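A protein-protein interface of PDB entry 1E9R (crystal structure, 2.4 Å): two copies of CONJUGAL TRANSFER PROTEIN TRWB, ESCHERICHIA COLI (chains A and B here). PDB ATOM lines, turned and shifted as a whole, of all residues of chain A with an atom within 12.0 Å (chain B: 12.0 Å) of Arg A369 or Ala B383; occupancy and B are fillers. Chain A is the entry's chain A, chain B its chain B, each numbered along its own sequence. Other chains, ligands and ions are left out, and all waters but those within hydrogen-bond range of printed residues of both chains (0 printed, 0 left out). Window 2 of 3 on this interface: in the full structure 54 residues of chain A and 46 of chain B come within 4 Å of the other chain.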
ATOM      1  N   VAL A   4      16.020 -14.508   4.989  1.00  0.00           N
ATOM      2  CA  VAL A   4      15.924 -13.525   6.106  1.00  0.00           C
ATOM      3  C   VAL A   4      14.472 -13.440   6.641  1.00  0.00           C
ATOM      4  O   VAL A   4      14.038 -12.408   7.167  1.00  0.00           O
ATOM      5  CB  VAL A   4      16.470 -12.133   5.616  1.00  0.00           C
ATOM      6  CG1 VAL A   4      15.779 -11.723   4.333  1.00  0.00           C
ATOM      7  CG2 VAL A   4      16.316 -11.071   6.695  1.00  0.00           C
ATOM      8  N   GLY A  11       8.139 -21.973   4.897  1.00  0.00           N
ATOM      9  CA  GLY A  11       8.603 -21.811   3.531  1.00  0.00           C
ATOM     10  C   GLY A  11       9.945 -21.120   3.460  1.00  0.00           C
ATOM     11  O   GLY A  11      10.679 -21.073   4.446  1.00  0.00           O
ATOM     12  N   ALA A  12      10.269 -20.582   2.292  1.00  0.00           N
ATOM     13  CA  ALA A  12      11.529 -19.881   2.092  1.00  0.00           C
ATOM     14  C   ALA A  12      11.534 -18.528   2.817  1.00  0.00           C
ATOM     15  O   ALA A  12      10.535 -17.790   2.805  1.00  0.00           O
ATOM     16  CB  ALA A  12      11.771 -19.675   0.600  1.00  0.00           C
ATOM     17  N   PRO A  13      12.658 -18.187   3.468  1.00  0.00           N
ATOM     18  CA  PRO A  13      12.758 -16.912   4.184  1.00  0.00           C
ATOM     19  C   PRO A  13      12.574 -15.770   3.195  1.00  0.00           C
ATOM     20  O   PRO A  13      12.898 -15.909   2.015  1.00  0.00           O
ATOM     21  CB  PRO A  13      14.167 -16.956   4.764  1.00  0.00           C
ATOM     22  CG  PRO A  13      14.400 -18.438   4.962  1.00  0.00           C
ATOM     23  CD  PRO A  13      13.862 -19.013   3.679  1.00  0.00           C
ATOM     24  N   PHE A  14      12.066 -14.641   3.666  1.00  0.00           N
ATOM     25  CA  PHE A  14      11.842 -13.518   2.773  1.00  0.00           C
ATOM     26  C   PHE A  14      12.377 -12.182   3.263  1.00  0.00           C
ATOM     27  O   PHE A  14      12.655 -11.996   4.451  1.00  0.00           O
ATOM     28  CB  PHE A  14      10.354 -13.393   2.487  1.00  0.00           C
ATOM     29  CG  PHE A  14       9.493 -13.424   3.722  1.00  0.00           C
ATOM     30  CD1 PHE A  14       9.143 -14.633   4.311  1.00  0.00           C
ATOM     31  CD2 PHE A  14       9.037 -12.239   4.296  1.00  0.00           C
ATOM     32  CE1 PHE A  14       8.348 -14.661   5.458  1.00  0.00           C
ATOM     33  CE2 PHE A  14       8.243 -12.258   5.439  1.00  0.00           C
ATOM     34  CZ  PHE A  14       7.898 -13.471   6.022  1.00  0.00           C
ATOM     35  N   LYS A  15      12.496 -11.245   2.331  1.00  0.00           N
ATOM     36  CA  LYS A  15      13.008  -9.919   2.629  1.00  0.00           C
ATOM     37  C   LYS A  15      11.970  -9.070   3.357  1.00  0.00           C
ATOM     38  O   LYS A  15      12.217  -8.597   4.464  1.00  0.00           O
ATOM     39  CB  LYS A  15      13.434  -9.236   1.323  1.00  0.00           C
ATOM     40  CG  LYS A  15      14.518  -8.161   1.475  1.00  0.00           C
ATOM     41  CD  LYS A  15      14.832  -7.496   0.130  1.00  0.00           C
ATOM     42  CE  LYS A  15      16.114  -6.668   0.183  1.00  0.00           C
ATOM     43  NZ  LYS A  15      16.073  -5.575   1.196  1.00  0.00           N
ATOM     44  N   ARG A  16      10.801  -8.896   2.746  1.00  0.00           N
ATOM     45  CA  ARG A  16       9.760  -8.071   3.348  1.00  0.00           C
ATOM     46  C   ARG A  16       8.360  -8.684   3.325  1.00  0.00           C
ATOM     47  O   ARG A  16       7.947  -9.288   2.337  1.00  0.00           O
ATOM     48  CB  ARG A  16       9.704  -6.710   2.639  1.00  0.00           C
ATOM     49  CG  ARG A  16       8.947  -5.648   3.424  1.00  0.00           C
ATOM     50  CD  ARG A  16       8.607  -4.401   2.622  1.00  0.00           C
ATOM     51  NE  ARG A  16       9.606  -4.029   1.630  1.00  0.00           N
ATOM     52  CZ  ARG A  16      10.767  -3.406   1.839  1.00  0.00           C
ATOM     53  NH1 ARG A  16      11.181  -3.033   3.046  1.00  0.00           N
ATOM     54  NH2 ARG A  16      11.520  -3.133   0.785  1.00  0.00           N
ATOM     55  N   VAL A 365       4.530 -11.641  -0.043  1.00  0.00           N
ATOM     56  CA  VAL A 365       5.871 -11.380   0.419  1.00  0.00           C
ATOM     57  C   VAL A 365       6.851 -11.015  -0.705  1.00  0.00           C
ATOM     58  O   VAL A 365       6.596 -11.320  -1.867  1.00  0.00           O
ATOM     59  CB  VAL A 365       6.320 -12.661   1.158  1.00  0.00           C
ATOM     60  CG1 VAL A 365       7.764 -12.770   1.199  1.00  0.00           C
ATOM     61  CG2 VAL A 365       5.774 -12.669   2.543  1.00  0.00           C
ATOM     62  N   GLU A 366       7.955 -10.346  -0.353  1.00  0.00           N
ATOM     63  CA  GLU A 366       8.995  -9.990  -1.325  1.00  0.00           C
ATOM     64  C   GLU A 366      10.232 -10.774  -0.947  1.00  0.00           C
ATOM     65  O   GLU A 366      10.643 -10.772   0.211  1.00  0.00           O
ATOM     66  CB  GLU A 366       9.338  -8.500  -1.283  1.00  0.00           C
ATOM     67  CG  GLU A 366       8.208  -7.590  -1.707  1.00  0.00           C
ATOM     68  CD  GLU A 366       8.648  -6.152  -1.900  1.00  0.00           C
ATOM     69  OE1 GLU A 366       9.432  -5.651  -1.064  1.00  0.00           O
ATOM     70  OE2 GLU A 366       8.196  -5.524  -2.885  1.00  0.00           O
ATOM     71  N   ARG A 367      10.822 -11.447  -1.923  1.00  0.00           N
ATOM     72  CA  ARG A 367      12.016 -12.242  -1.661  1.00  0.00           C
ATOM     73  C   ARG A 367      13.145 -11.935  -2.633  1.00  0.00           C
ATOM     74  O   ARG A 367      12.919 -11.402  -3.720  1.00  0.00           O
ATOM     75  CB  ARG A 367      11.683 -13.733  -1.742  1.00  0.00           C
ATOM     76  CG  ARG A 367      11.802 -14.474  -0.423  1.00  0.00           C
ATOM     77  CD  ARG A 367      11.760 -15.977  -0.647  1.00  0.00           C
ATOM     78  NE  ARG A 367      10.506 -16.415  -1.242  1.00  0.00           N
ATOM     79  CZ  ARG A 367       9.418 -16.720  -0.545  1.00  0.00           C
ATOM     80  NH1 ARG A 367       9.423 -16.644   0.781  1.00  0.00           N
ATOM     81  NH2 ARG A 367       8.317 -17.091  -1.179  1.00  0.00           N
ATOM     82  N   ASP A 368      14.365 -12.268  -2.224  1.00  0.00           N
ATOM     83  CA  ASP A 368      15.535 -12.065  -3.071  1.00  0.00           C
ATOM     84  C   ASP A 368      15.635 -13.269  -4.007  1.00  0.00           C
ATOM     85  O   ASP A 368      15.770 -14.398  -3.545  1.00  0.00           O
ATOM     86  CB  ASP A 368      16.797 -11.951  -2.207  1.00  0.00           C
ATOM     87  CG  ASP A 368      16.912 -10.599  -1.515  1.00  0.00           C
ATOM     88  OD1 ASP A 368      16.273  -9.632  -1.986  1.00  0.00           O
ATOM     89  OD2 ASP A 368      17.653 -10.497  -0.510  1.00  0.00           O
ATOM     90  N   ARG A 369      15.518 -13.005  -5.310  1.00  0.00           N
ATOM     91  CA  ARG A 369      15.588 -14.000  -6.398  1.00  0.00           C
ATOM     92  C   ARG A 369      14.665 -13.588  -7.550  1.00  0.00           C
ATOM     93  O   ARG A 369      13.879 -14.439  -8.022  1.00  0.00           O
ATOM     94  CB  ARG A 369      15.198 -15.425  -5.933  1.00  0.00           C
ATOM     95  CG  ARG A 369      16.339 -16.291  -5.340  1.00  0.00           C
ATOM     96  CD  ARG A 369      17.493 -16.532  -6.315  1.00  0.00           C
ATOM     97  NE  ARG A 369      18.159 -15.285  -6.692  1.00  0.00           N
ATOM     98  CZ  ARG A 369      18.823 -14.495  -5.850  1.00  0.00           C
ATOM     99  NH1 ARG A 369      18.937 -14.826  -4.568  1.00  0.00           N
ATOM    100  NH2 ARG A 369      19.387 -13.378  -6.295  1.00  0.00           N
ATOM    101  N   ALA A 383      17.230  -7.866  -8.078  1.00  0.00           N
ATOM    102  CA  ALA A 383      15.815  -8.109  -8.485  1.00  0.00           C
ATOM    103  C   ALA A 383      15.040  -8.821  -7.372  1.00  0.00           C
ATOM    104  O   ALA A 383      15.500  -9.834  -6.840  1.00  0.00           O
ATOM    105  CB  ALA A 383      15.779  -8.943  -9.768  1.00  0.00           C
ATOM    106  N   LEU A 384      13.871  -8.276  -7.023  1.00  0.00           N
ATOM    107  CA  LEU A 384      12.989  -8.833  -5.988  1.00  0.00           C
ATOM    108  C   LEU A 384      11.740  -9.430  -6.624  1.00  0.00           C
ATOM    109  O   LEU A 384      11.310  -8.974  -7.687  1.00  0.00           O
ATOM    110  CB  LEU A 384      12.550  -7.749  -4.993  1.00  0.00           C
ATOM    111  CG  LEU A 384      13.475  -7.351  -3.836  1.00  0.00           C
ATOM    112  CD1 LEU A 384      12.796  -6.288  -2.996  1.00  0.00           C
ATOM    113  CD2 LEU A 384      13.795  -8.557  -2.967  1.00  0.00           C
ATOM    114  N   GLU A 385      11.158 -10.439  -5.973  1.00  0.00           N
ATOM    115  CA  GLU A 385       9.945 -11.083  -6.475  1.00  0.00           C
ATOM    116  C   GLU A 385       8.804 -11.006  -5.462  1.00  0.00           C
ATOM    117  O   GLU A 385       9.007 -11.238  -4.268  1.00  0.00           O
ATOM    118  CB  GLU A 385      10.210 -12.551  -6.812  1.00  0.00           C
ATOM    119  CG  GLU A 385      10.534 -13.400  -5.603  1.00  0.00           C
ATOM    120  CD  GLU A 385      10.322 -14.885  -5.850  1.00  0.00           C
ATOM    121  OE1 GLU A 385       9.974 -15.266  -6.993  1.00  0.00           O
ATOM    122  OE2 GLU A 385      10.503 -15.671  -4.894  1.00  0.00           O
ATOM    123  N   ARG A 386       7.612 -10.662  -5.951  1.00  0.00           N
ATOM    124  CA  ARG A 386       6.411 -10.568  -5.122  1.00  0.00           C
ATOM    125  C   ARG A 386       5.690 -11.903  -5.238  1.00  0.00           C
ATOM    126  O   ARG A 386       5.331 -12.322  -6.335  1.00  0.00           O
ATOM    127  CB  ARG A 386       5.480  -9.464  -5.628  1.00  0.00           C
ATOM    128  CG  ARG A 386       5.347  -8.293  -4.692  1.00  0.00           C
ATOM    129  CD  ARG A 386       5.775  -7.004  -5.371  1.00  0.00           C
ATOM    130  NE  ARG A 386       7.176  -7.005  -5.782  1.00  0.00           N
ATOM    131  CZ  ARG A 386       7.795  -5.962  -6.326  1.00  0.00           C
ATOM    132  NH1 ARG A 386       7.140  -4.826  -6.522  1.00  0.00           N
ATOM    133  NH2 ARG A 386       9.068  -6.055  -6.686  1.00  0.00           N
ATOM    134  N   VAL A 387       5.469 -12.569  -4.113  1.00  0.00           N
ATOM    135  CA  VAL A 387       4.811 -13.864  -4.144  1.00  0.00           C
ATOM    136  C   VAL A 387       3.738 -14.034  -3.083  1.00  0.00           C
ATOM    137  O   VAL A 387       3.893 -13.582  -1.945  1.00  0.00           O
ATOM    138  CB  VAL A 387       5.847 -15.004  -3.975  1.00  0.00           C
ATOM    139  CG1 VAL A 387       5.152 -16.335  -3.814  1.00  0.00           C
ATOM    140  CG2 VAL A 387       6.759 -15.052  -5.181  1.00  0.00           C
ATOM    141  N   GLU A 389       1.528 -16.847  -1.033  1.00  0.00           N
ATOM    142  CA  GLU A 389       1.629 -18.253  -0.652  1.00  0.00           C
ATOM    143  C   GLU A 389       0.949 -18.556   0.677  1.00  0.00           C
ATOM    144  O   GLU A 389       0.693 -17.656   1.484  1.00  0.00           O
ATOM    145  CB  GLU A 389       3.099 -18.677  -0.586  1.00  0.00           C
ATOM    146  CG  GLU A 389       4.024 -17.567  -0.136  1.00  0.00           C
ATOM    147  CD  GLU A 389       5.458 -18.023   0.029  1.00  0.00           C
ATOM    148  OE1 GLU A 389       5.970 -18.734  -0.863  1.00  0.00           O
ATOM    149  OE2 GLU A 389       6.077 -17.659   1.047  1.00  0.00           O
ATOM    150  N   ASN B   2      21.996 -30.293  -5.953  1.00  0.00           N
ATOM    151  CA  ASN B   2      20.762 -31.132  -5.953  1.00  0.00           C
ATOM    152  C   ASN B   2      21.096 -32.564  -5.534  1.00  0.00           C
ATOM    153  O   ASN B   2      20.924 -33.508  -6.308  1.00  0.00           O
ATOM    154  CB  ASN B   2      20.113 -31.138  -7.347  1.00  0.00           C
ATOM    155  CG  ASN B   2      19.761 -29.741  -7.843  1.00  0.00           C
ATOM    156  OD1 ASN B   2      19.121 -28.960  -7.139  1.00  0.00           O
ATOM    157  ND2 ASN B   2      20.172 -29.426  -9.067  1.00  0.00           N
ATOM    158  N   PRO B  13      15.807 -34.224  -8.745  1.00  0.00           N
ATOM    159  CA  PRO B  13      16.546 -34.037  -7.492  1.00  0.00           C
ATOM    160  C   PRO B  13      16.581 -32.551  -7.122  1.00  0.00           C
ATOM    161  O   PRO B  13      16.556 -31.690  -8.003  1.00  0.00           O
ATOM    162  CB  PRO B  13      17.931 -34.589  -7.825  1.00  0.00           C
ATOM    163  CG  PRO B  13      17.618 -35.681  -8.815  1.00  0.00           C
ATOM    164  CD  PRO B  13      16.598 -35.008  -9.712  1.00  0.00           C
ATOM    165  N   PHE B  14      16.621 -32.253  -5.827  1.00  0.00           N
ATOM    166  CA  PHE B  14      16.646 -30.872  -5.382  1.00  0.00           C
ATOM    167  C   PHE B  14      17.747 -30.539  -4.383  1.00  0.00           C
ATOM    168  O   PHE B  14      18.356 -31.421  -3.775  1.00  0.00           O
ATOM    169  CB  PHE B  14      15.296 -30.474  -4.791  1.00  0.00           C
ATOM    170  CG  PHE B  14      14.775 -31.416  -3.739  1.00  0.00           C
ATOM    171  CD1 PHE B  14      14.078 -32.569  -4.102  1.00  0.00           C
ATOM    172  CD2 PHE B  14      14.937 -31.129  -2.382  1.00  0.00           C
ATOM    173  CE1 PHE B  14      13.538 -33.426  -3.129  1.00  0.00           C
ATOM    174  CE2 PHE B  14      14.405 -31.975  -1.405  1.00  0.00           C
ATOM    175  CZ  PHE B  14      13.699 -33.131  -1.782  1.00  0.00           C
ATOM    176  N   LYS B  15      17.982 -29.243  -4.214  1.00  0.00           N
ATOM    177  CA  LYS B  15      19.011 -28.755  -3.315  1.00  0.00           C
ATOM    178  C   LYS B  15      18.530 -28.791  -1.878  1.00  0.00           C
ATOM    179  O   LYS B  15      19.134 -29.459  -1.040  1.00  0.00           O
ATOM    180  CB  LYS B  15      19.399 -27.318  -3.693  1.00  0.00           C
ATOM    181  CG  LYS B  15      20.819 -26.896  -3.299  1.00  0.00           C
ATOM    182  CD  LYS B  15      21.078 -25.427  -3.674  1.00  0.00           C
ATOM    183  CE  LYS B  15      22.568 -25.063  -3.652  1.00  0.00           C
ATOM    184  NZ  LYS B  15      23.197 -25.259  -2.315  1.00  0.00           N
ATOM    185  N   ARG B  16      17.426 -28.100  -1.603  1.00  0.00           N
ATOM    186  CA  ARG B  16      16.897 -28.013  -0.244  1.00  0.00           C
ATOM    187  C   ARG B  16      15.405 -28.243  -0.072  1.00  0.00           C
ATOM    188  O   ARG B  16      14.594 -27.707  -0.817  1.00  0.00           O
ATOM    189  CB  ARG B  16      17.238 -26.648   0.335  1.00  0.00           C
ATOM    190  CG  ARG B  16      16.538 -26.305   1.635  1.00  0.00           C
ATOM    191  CD  ARG B  16      16.995 -24.931   2.099  1.00  0.00           C
ATOM    192  NE  ARG B  16      18.437 -24.972   2.303  1.00  0.00           N
ATOM    193  CZ  ARG B  16      19.307 -24.013   1.997  1.00  0.00           C
ATOM    194  NH1 ARG B  16      18.912 -22.870   1.447  1.00  0.00           N
ATOM    195  NH2 ARG B  16      20.596 -24.214   2.247  1.00  0.00           N
ATOM    196  N   LEU B  18      12.045 -27.621   1.877  1.00  0.00           N
ATOM    197  CA  LEU B  18      11.507 -26.549   2.704  1.00  0.00           C
ATOM    198  C   LEU B  18      10.366 -26.972   3.616  1.00  0.00           C
ATOM    199  O   LEU B  18      10.471 -26.880   4.830  1.00  0.00           O
ATOM    200  CB  LEU B  18      11.040 -25.389   1.824  1.00  0.00           C
ATOM    201  CG  LEU B  18      12.154 -24.598   1.146  1.00  0.00           C
ATOM    202  CD1 LEU B  18      11.585 -23.595   0.148  1.00  0.00           C
ATOM    203  CD2 LEU B  18      12.949 -23.895   2.229  1.00  0.00           C
ATOM    204  N   VAL B 365      10.159 -27.057  -2.352  1.00  0.00           N
ATOM    205  CA  VAL B 365      11.565 -27.386  -2.500  1.00  0.00           C
ATOM    206  C   VAL B 365      12.356 -26.341  -3.304  1.00  0.00           C
ATOM    207  O   VAL B 365      11.773 -25.587  -4.075  1.00  0.00           O
ATOM    208  CB  VAL B 365      11.608 -28.786  -3.196  1.00  0.00           C
ATOM    209  CG1 VAL B 365      12.776 -28.901  -4.102  1.00  0.00           C
ATOM    210  CG2 VAL B 365      11.582 -29.892  -2.153  1.00  0.00           C
ATOM    211  N   GLU B 366      13.678 -26.287  -3.110  1.00  0.00           N
ATOM    212  CA  GLU B 366      14.540 -25.362  -3.865  1.00  0.00           C
ATOM    213  C   GLU B 366      15.439 -26.197  -4.767  1.00  0.00           C
ATOM    214  O   GLU B 366      16.049 -27.169  -4.311  1.00  0.00           O
ATOM    215  CB  GLU B 366      15.409 -24.510  -2.938  1.00  0.00           C
ATOM    216  CG  GLU B 366      14.618 -23.630  -2.000  1.00  0.00           C
ATOM    217  CD  GLU B 366      15.487 -22.672  -1.212  1.00  0.00           C
ATOM    218  OE1 GLU B 366      16.557 -23.097  -0.723  1.00  0.00           O
ATOM    219  OE2 GLU B 366      15.090 -21.496  -1.068  1.00  0.00           O
ATOM    220  N   ARG B 367      15.520 -25.818  -6.041  1.00  0.00           N
ATOM    221  CA  ARG B 367      16.330 -26.546  -7.017  1.00  0.00           C
ATOM    222  C   ARG B 367      17.280 -25.678  -7.841  1.00  0.00           C
ATOM    223  O   ARG B 367      17.013 -24.503  -8.083  1.00  0.00           O
ATOM    224  CB  ARG B 367      15.418 -27.302  -7.977  1.00  0.00           C
ATOM    225  CG  ARG B 367      15.495 -28.796  -7.853  1.00  0.00           C
ATOM    226  CD  ARG B 367      14.887 -29.435  -9.068  1.00  0.00           C
ATOM    227  NE  ARG B 367      13.458 -29.172  -9.157  1.00  0.00           N
ATOM    228  CZ  ARG B 367      12.522 -29.862  -8.509  1.00  0.00           C
ATOM    229  NH1 ARG B 367      12.849 -30.873  -7.710  1.00  0.00           N
ATOM    230  NH2 ARG B 367      11.246 -29.539  -8.669  1.00  0.00           N
ATOM    231  N   ASP B 368      18.386 -26.273  -8.280  1.00  0.00           N
ATOM    232  CA  ASP B 368      19.357 -25.565  -9.104  1.00  0.00           C
ATOM    233  C   ASP B 368      18.792 -25.509 -10.505  1.00  0.00           C
ATOM    234  O   ASP B 368      18.438 -26.539 -11.071  1.00  0.00           O
ATOM    235  CB  ASP B 368      20.695 -26.307  -9.121  1.00  0.00           C
ATOM    236  CG  ASP B 368      21.528 -26.040  -7.874  1.00  0.00           C
ATOM    237  OD1 ASP B 368      21.184 -25.105  -7.117  1.00  0.00           O
ATOM    238  OD2 ASP B 368      22.532 -26.757  -7.653  1.00  0.00           O
ATOM    239  N   ARG B 369      18.712 -24.310 -11.069  1.00  0.00           N
ATOM    240  CA  ARG B 369      18.163 -24.147 -12.411  1.00  0.00           C
ATOM    241  C   ARG B 369      19.022 -24.706 -13.560  1.00  0.00           C
ATOM    242  O   ARG B 369      18.497 -24.998 -14.640  1.00  0.00           O
ATOM    243  CB  ARG B 369      17.853 -22.668 -12.662  1.00  0.00           C
ATOM    244  CG  ARG B 369      16.864 -22.087 -11.674  1.00  0.00           C
ATOM    245  CD  ARG B 369      16.338 -20.744 -12.148  1.00  0.00           C
ATOM    246  NE  ARG B 369      15.257 -20.245 -11.297  1.00  0.00           N
ATOM    247  CZ  ARG B 369      14.471 -19.211 -11.603  1.00  0.00           C
ATOM    248  NH1 ARG B 369      14.637 -18.560 -12.750  1.00  0.00           N
ATOM    249  NH2 ARG B 369      13.513 -18.829 -10.763  1.00  0.00           N
ATOM    250  N   TYR B 370      20.328 -24.870 -13.333  1.00  0.00           N
ATOM    251  CA  TYR B 370      21.222 -25.386 -14.375  1.00  0.00           C
ATOM    252  C   TYR B 370      21.707 -26.815 -14.110  1.00  0.00           C
ATOM    253  O   TYR B 370      21.652 -27.251 -12.936  1.00  0.00           O
ATOM    254  CB  TYR B 370      22.434 -24.461 -14.532  1.00  0.00           C
ATOM    255  CG  TYR B 370      22.053 -23.016 -14.722  1.00  0.00           C
ATOM    256  CD1 TYR B 370      21.442 -22.300 -13.688  1.00  0.00           C
ATOM    257  CD2 TYR B 370      22.253 -22.375 -15.944  1.00  0.00           C
ATOM    258  CE1 TYR B 370      21.037 -20.988 -13.862  1.00  0.00           C
ATOM    259  CE2 TYR B 370      21.851 -21.057 -16.131  1.00  0.00           C
ATOM    260  CZ  TYR B 370      21.239 -20.372 -15.084  1.00  0.00           C
ATOM    261  OH  TYR B 370      20.812 -19.078 -15.258  1.00  0.00           O
ATOM    262  N   ALA B 383      20.278 -18.210  -8.640  1.00  0.00           N
ATOM    263  CA  ALA B 383      19.904 -19.183  -9.707  1.00  0.00           C
ATOM    264  C   ALA B 383      19.109 -20.352  -9.119  1.00  0.00           C
ATOM    265  O   ALA B 383      19.071 -21.450  -9.693  1.00  0.00           O
ATOM    266  CB  ALA B 383      21.162 -19.700 -10.406  1.00  0.00           C
ATOM    267  N   LEU B 384      18.482 -20.115  -7.968  1.00  0.00           N
ATOM    268  CA  LEU B 384      17.681 -21.147  -7.316  1.00  0.00           C
ATOM    269  C   LEU B 384      16.196 -20.910  -7.544  1.00  0.00           C
ATOM    270  O   LEU B 384      15.742 -19.766  -7.589  1.00  0.00           O
ATOM    271  CB  LEU B 384      17.957 -21.191  -5.807  1.00  0.00           C
ATOM    272  CG  LEU B 384      19.160 -21.990  -5.293  1.00  0.00           C
ATOM    273  CD1 LEU B 384      19.150 -21.980  -3.772  1.00  0.00           C
ATOM    274  CD2 LEU B 384      19.099 -23.423  -5.796  1.00  0.00           C
ATOM    275  N   GLU B 385      15.447 -22.000  -7.678  1.00  0.00           N
ATOM    276  CA  GLU B 385      14.009 -21.928  -7.903  1.00  0.00           C
ATOM    277  C   GLU B 385      13.221 -22.613  -6.791  1.00  0.00           C
ATOM    278  O   GLU B 385      13.556 -23.719  -6.379  1.00  0.00           O
ATOM    279  CB  GLU B 385      13.659 -22.585  -9.237  1.00  0.00           C
ATOM    280  CG  GLU B 385      14.006 -24.065  -9.316  1.00  0.00           C
ATOM    281  CD  GLU B 385      13.386 -24.746 -10.530  1.00  0.00           C
ATOM    282  OE1 GLU B 385      12.688 -24.056 -11.304  1.00  0.00           O
ATOM    283  OE2 GLU B 385      13.589 -25.969 -10.714  1.00  0.00           O
ATOM    284  N   ARG B 386      12.175 -21.945  -6.310  1.00  0.00           N
ATOM    285  CA  ARG B 386      11.319 -22.494  -5.264  1.00  0.00           C
ATOM    286  C   ARG B 386      10.107 -23.092  -5.964  1.00  0.00           C
ATOM    287  O   ARG B 386       9.417 -22.412  -6.714  1.00  0.00           O
ATOM    288  CB  ARG B 386      10.898 -21.394  -4.296  1.00  0.00           C
ATOM    289  CG  ARG B 386       9.850 -21.804  -3.294  1.00  0.00           C
ATOM    290  CD  ARG B 386       9.677 -20.706  -2.265  1.00  0.00           C
ATOM    291  NE  ARG B 386       9.748 -19.365  -2.859  1.00  0.00           N
ATOM    292  CZ  ARG B 386       8.845 -18.851  -3.695  1.00  0.00           C
ATOM    293  NH1 ARG B 386       7.771 -19.556  -4.049  1.00  0.00           N
ATOM    294  NH2 ARG B 386       9.012 -17.624  -4.174  1.00  0.00           N
ATOM    295  N   VAL B 387       9.848 -24.371  -5.717  1.00  0.00           N
ATOM    296  CA  VAL B 387       8.755 -25.061  -6.383  1.00  0.00           C
ATOM    297  C   VAL B 387       7.906 -25.932  -5.472  1.00  0.00           C
ATOM    298  O   VAL B 387       8.420 -26.589  -4.570  1.00  0.00           O
ATOM    299  CB  VAL B 387       9.319 -25.955  -7.528  1.00  0.00           C
ATOM    300  CG1 VAL B 387       8.240 -26.837  -8.109  1.00  0.00           C
ATOM    301  CG2 VAL B 387       9.904 -25.083  -8.618  1.00  0.00           C
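Of the 18 printed residues of chain A, 6 touch a printed residue of chain B. Hydrophobic or aromatic side chains of chain A within 4 Å of the printed part of chain B: Ala A12 and Val A387. Along chain B the printed residues that touch a printed residue of chain A span positions 18 to 386. Among the printed residues, Asp or Glu carboxylates within 4 Å of a Lys or Arg side-chain nitrogen of the other chain: Glu A385 with Arg B386 (2.6 Å) and Glu A389 with Arg B386 (3.8 Å).
Arg A369 touches Ala B383, but with the chains exchanged Ala A383 does not touch Arg B369 (10.0 Å). Arg A369 touches Leu B384, but with the chains exchanged Leu A384 does not touch Arg B369 (10.4 Å). Glu A385 touches Arg B386, but with the chains exchanged Arg A386 does not touch Glu B385 (13.0 Å). Val A387 touches Arg B386, but with the chains exchanged Arg A386 does not touch Val B387 (12.9 Å). Positions printed for both chains: 13, 14, 15, 16, 365, 366, 367, 368, 369, 383, 384, 385, 386 and 387.
The side-chain carboxylate (OE2) of Glu A385 lies within salt-bridge range of the guanidinium group (NH2) of Arg B386. OE1 of Glu A389 lies within salt-bridge range of NH1 of Arg B386 (3.8 Å). The guanidinium group (NH2) of Arg A367 sits close to the guanidinium group (NH2) of Arg B386.
Among the printed residues, merely in contact across the chains: Val A387 with Arg B386 (3.6 Å), Ala A12 with Arg B386 (3.7 Å), Arg A369 with Leu B384 (3.9 Å), Ala A12 with Leu B18 (3.9 Å) and Arg A369 with Ala B383 (3.997 Å).
The backbone carbonyl oxygen (O) of Val A387 lies within hydrogen-bond range of the backbone NH (N) of Val A365 (2.8 Å). The backbone carbonyl oxygen of Ala A12 sits at hydrogen-bond distance from the guanidinium group of Arg A367 (2.6 Å). The guanidinium group (NH2) of Arg A367 lies within salt-bridge range of the side-chain carboxylate (OE1) of Glu A389 (2.9 Å). The backbone NH of Arg B369 lies close to the backbone carbonyl oxygen of Ala B383 (3.2 Å). OE2 of Glu A385 is in salt-bridge range of NE of Arg A367, at 3.7 Å.
Printed residues of chain B within 4 Å of Ala A12: Leu B18 and Arg B386. Val A365 touches none of the printed residues of chain B. Printed residues of chain B within 4 Å of Arg A369: Ala B383 (3.997 Å) and Leu B384 (3.9 Å). Of the printed residues of chain B, Glu A385 touches Arg B386. Printed residues of chain B within 4 Å of Val A387: Arg B386 (3.6 Å). Printed residues of chain B within 4 Å of Glu A389: Arg B386 (3.8 Å). Printed residues of chain A within 4 Å of Leu B18: Ala A12. Glu B366 touches none of the printed residues of chain A. No residue of chain A comes within 4 Å of Asp B368. No residue of chain A comes within 4 Å of Arg B369. No residue of chain A comes within 4 Å of Tyr B370. Printed residues of chain A within 4 Å of Ala B383: Arg A369 (3.997 Å). Leu B384 touches one residue of chain A. No residue of chain A comes within 4 Å of Glu B385. Of the printed residues of chain A, Arg B386 touches Ala A12, Arg A367, Glu A385, Val A387 and Glu A389. The nearest printed residue of chain B that does not touch Arg A369 is Arg B369 (5.2 Å). The nearest printed residue of chain A that does not touch Ala B383 is Asp A368 (7.8 Å). The nearest printed residue of chain A that does not touch Leu B18 is Gly A11 (4.2 Å).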
